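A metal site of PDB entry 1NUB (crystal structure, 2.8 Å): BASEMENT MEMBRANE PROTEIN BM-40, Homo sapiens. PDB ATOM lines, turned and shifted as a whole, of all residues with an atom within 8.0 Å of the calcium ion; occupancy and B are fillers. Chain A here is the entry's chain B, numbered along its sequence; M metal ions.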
ATOM      1  N   LYS A  84       1.069 -31.207  -7.213  1.00  0.00           N
ATOM      2  CA  LYS A  84       0.071 -30.770  -8.164  1.00  0.00           C
ATOM      3  C   LYS A  84      -0.229 -31.856  -9.183  1.00  0.00           C
ATOM      4  O   LYS A  84       0.480 -32.855  -9.260  1.00  0.00           O
ATOM      5  CB  LYS A  84       0.618 -29.548  -8.899  1.00  0.00           C
ATOM      6  CG  LYS A  84       1.938 -29.750  -9.617  1.00  0.00           C
ATOM      7  CD  LYS A  84       2.255 -28.556 -10.467  1.00  0.00           C
ATOM      8  CE  LYS A  84       3.432 -28.820 -11.374  1.00  0.00           C
ATOM      9  NZ  LYS A  84       3.426 -27.879 -12.529  1.00  0.00           N
ATOM     10  N   TRP A 104      17.498 -27.981 -25.296  1.00  0.00           N
ATOM     11  CA  TRP A 104      17.189 -27.092 -24.181  1.00  0.00           C
ATOM     12  C   TRP A 104      18.469 -26.898 -23.368  1.00  0.00           C
ATOM     13  O   TRP A 104      18.835 -25.774 -23.051  1.00  0.00           O
ATOM     14  CB  TRP A 104      16.103 -27.707 -23.292  1.00  0.00           C
ATOM     15  CG  TRP A 104      15.624 -26.792 -22.203  1.00  0.00           C
ATOM     16  CD1 TRP A 104      14.779 -25.721 -22.334  1.00  0.00           C
ATOM     17  CD2 TRP A 104      15.980 -26.848 -20.818  1.00  0.00           C
ATOM     18  NE1 TRP A 104      14.596 -25.109 -21.120  1.00  0.00           N
ATOM     19  CE2 TRP A 104      15.327 -25.774 -20.173  1.00  0.00           C
ATOM     20  CE3 TRP A 104      16.795 -27.700 -20.059  1.00  0.00           C
ATOM     21  CZ2 TRP A 104      15.469 -25.535 -18.810  1.00  0.00           C
ATOM     22  CZ3 TRP A 104      16.923 -27.462 -18.717  1.00  0.00           C
ATOM     23  CH2 TRP A 104      16.263 -26.397 -18.091  1.00  0.00           C
ATOM     24  N   LEU A 181      15.093 -31.211 -12.863  1.00  0.00           N
ATOM     25  CA  LEU A 181      14.604 -31.444 -14.205  1.00  0.00           C
ATOM     26  C   LEU A 181      13.094 -31.656 -14.291  1.00  0.00           C
ATOM     27  O   LEU A 181      12.556 -31.847 -15.386  1.00  0.00           O
ATOM     28  CB  LEU A 181      15.364 -32.596 -14.864  1.00  0.00           C
ATOM     29  CG  LEU A 181      16.799 -32.226 -15.239  1.00  0.00           C
ATOM     30  CD1 LEU A 181      17.483 -33.375 -15.970  1.00  0.00           C
ATOM     31  CD2 LEU A 181      16.770 -31.001 -16.129  1.00  0.00           C
ATOM     32  N   ARG A 182      12.407 -31.575 -13.151  1.00  0.00           N
ATOM     33  CA  ARG A 182      10.959 -31.746 -13.157  1.00  0.00           C
ATOM     34  C   ARG A 182      10.253 -30.410 -13.009  1.00  0.00           C
ATOM     35  O   ARG A 182       9.031 -30.365 -12.832  1.00  0.00           O
ATOM     36  CB  ARG A 182      10.521 -32.714 -12.053  1.00  0.00           C
ATOM     37  CG  ARG A 182      10.961 -34.142 -12.303  1.00  0.00           C
ATOM     38  CD  ARG A 182      10.538 -35.096 -11.218  1.00  0.00           C
ATOM     39  NE  ARG A 182      11.243 -36.375 -11.350  1.00  0.00           N
ATOM     40  CZ  ARG A 182      12.209 -36.784 -10.532  1.00  0.00           C
ATOM     41  NH1 ARG A 182      12.575 -36.031  -9.503  1.00  0.00           N
ATOM     42  NH2 ARG A 182      12.874 -37.900 -10.794  1.00  0.00           N
ATOM     43  N   ALA A 183      11.019 -29.329 -13.120  1.00  0.00           N
ATOM     44  CA  ALA A 183      10.476 -27.972 -12.999  1.00  0.00           C
ATOM     45  C   ALA A 183       9.726 -27.564 -14.242  1.00  0.00           C
ATOM     46  O   ALA A 183      10.088 -27.970 -15.333  1.00  0.00           O
ATOM     47  CB  ALA A 183      11.594 -26.988 -12.725  1.00  0.00           C
ATOM     48  N   PRO A 184       8.747 -26.662 -14.106  1.00  0.00           N
ATOM     49  CA  PRO A 184       7.907 -26.147 -15.198  1.00  0.00           C
ATOM     50  C   PRO A 184       8.627 -25.602 -16.423  1.00  0.00           C
ATOM     51  O   PRO A 184       8.059 -25.539 -17.512  1.00  0.00           O
ATOM     52  CB  PRO A 184       7.091 -25.066 -14.527  1.00  0.00           C
ATOM     53  CG  PRO A 184       6.934 -25.613 -13.148  1.00  0.00           C
ATOM     54  CD  PRO A 184       8.316 -26.084 -12.827  1.00  0.00           C
ATOM     55  N   LEU A 185       9.857 -25.153 -16.236  1.00  0.00           N
ATOM     56  CA  LEU A 185      10.623 -24.594 -17.340  1.00  0.00           C
ATOM     57  C   LEU A 185      11.114 -25.671 -18.290  1.00  0.00           C
ATOM     58  O   LEU A 185      11.206 -25.462 -19.492  1.00  0.00           O
ATOM     59  CB  LEU A 185      11.807 -23.765 -16.816  1.00  0.00           C
ATOM     60  CG  LEU A 185      12.353 -22.689 -17.754  1.00  0.00           C
ATOM     61  CD1 LEU A 185      11.284 -21.639 -18.009  1.00  0.00           C
ATOM     62  CD2 LEU A 185      13.600 -22.059 -17.136  1.00  0.00           C
ATOM     63  N   ILE A 186      11.441 -26.836 -17.746  1.00  0.00           N
ATOM     64  CA  ILE A 186      11.914 -27.948 -18.554  1.00  0.00           C
ATOM     65  C   ILE A 186      10.824 -28.351 -19.571  1.00  0.00           C
ATOM     66  O   ILE A 186       9.628 -28.340 -19.261  1.00  0.00           O
ATOM     67  CB  ILE A 186      12.318 -29.149 -17.656  1.00  0.00           C
ATOM     68  CG1 ILE A 186      13.679 -28.872 -17.006  1.00  0.00           C
ATOM     69  CG2 ILE A 186      12.403 -30.426 -18.464  1.00  0.00           C
ATOM     70  CD1 ILE A 186      13.690 -27.687 -16.080  1.00  0.00           C
ATOM     71  N   PRO A 187      11.210 -28.644 -20.807  1.00  0.00           N
ATOM     72  CA  PRO A 187      10.183 -29.037 -21.783  1.00  0.00           C
ATOM     73  C   PRO A 187       9.749 -30.485 -21.543  1.00  0.00           C
ATOM     74  O   PRO A 187      10.575 -31.400 -21.522  1.00  0.00           O
ATOM     75  CB  PRO A 187      10.908 -28.866 -23.107  1.00  0.00           C
ATOM     76  CG  PRO A 187      12.310 -29.271 -22.759  1.00  0.00           C
ATOM     77  CD  PRO A 187      12.541 -28.587 -21.439  1.00  0.00           C
ATOM     78  N   MET A 188       8.450 -30.672 -21.335  1.00  0.00           N
ATOM     79  CA  MET A 188       7.874 -31.993 -21.095  1.00  0.00           C
ATOM     80  C   MET A 188       8.497 -32.585 -19.835  1.00  0.00           C
ATOM     81  O   MET A 188       8.851 -33.763 -19.790  1.00  0.00           O
ATOM     82  CB  MET A 188       8.143 -32.929 -22.279  1.00  0.00           C
ATOM     83  CG  MET A 188       7.429 -32.558 -23.560  1.00  0.00           C
ATOM     84  SD  MET A 188       7.937 -33.610 -24.951  1.00  0.00           S
ATOM     85  CE  MET A 188       6.504 -33.476 -25.966  1.00  0.00           C
ATOM     86  N   GLU A 189       8.558 -31.769 -18.786  1.00  0.00           N
ATOM     87  CA  GLU A 189       9.152 -32.191 -17.526  1.00  0.00           C
ATOM     88  C   GLU A 189       8.447 -33.417 -16.964  1.00  0.00           C
ATOM     89  O   GLU A 189       9.080 -34.249 -16.321  1.00  0.00           O
ATOM     90  CB  GLU A 189       9.155 -31.050 -16.507  1.00  0.00           C
ATOM     91  CG  GLU A 189       7.794 -30.699 -15.920  1.00  0.00           C
ATOM     92  CD  GLU A 189       6.966 -29.752 -16.764  1.00  0.00           C
ATOM     93  OE1 GLU A 189       7.319 -29.504 -17.941  1.00  0.00           O
ATOM     94  OE2 GLU A 189       5.925 -29.256 -16.267  1.00  0.00           O
ATOM     95  N   HIS A 190       7.161 -33.561 -17.269  1.00  0.00           N
ATOM     96  CA  HIS A 190       6.386 -34.708 -16.794  1.00  0.00           C
ATOM     97  C   HIS A 190       6.904 -36.053 -17.347  1.00  0.00           C
ATOM     98  O   HIS A 190       6.490 -37.106 -16.878  1.00  0.00           O
ATOM     99  CB  HIS A 190       4.900 -34.542 -17.101  1.00  0.00           C
ATOM    100  CG  HIS A 190       4.583 -34.611 -18.557  1.00  0.00           C
ATOM    101  ND1 HIS A 190       4.375 -33.501 -19.336  1.00  0.00           N
ATOM    102  CD2 HIS A 190       4.483 -35.678 -19.402  1.00  0.00           C
ATOM    103  CE1 HIS A 190       4.167 -33.855 -20.584  1.00  0.00           C
ATOM    104  NE2 HIS A 190       4.228 -35.168 -20.649  1.00  0.00           N
HETATM  105 CA    CA M   1       7.458 -27.382 -19.018  1.00  0.00          CA
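The side-chain carboxylate (OE1) of Glu 189 binds the calcium ion. The backbone carbonyl oxygen (O) of Ile 186 is bound to the calcium ion. The backbone carbonyl oxygen (O) of Pro 184 binds the calcium ion, at 2.5 Å. The calcium ion has three donor atoms within binding distance.
Of the 12 residues printed, 3 come within 4 Å of the calcium ion.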
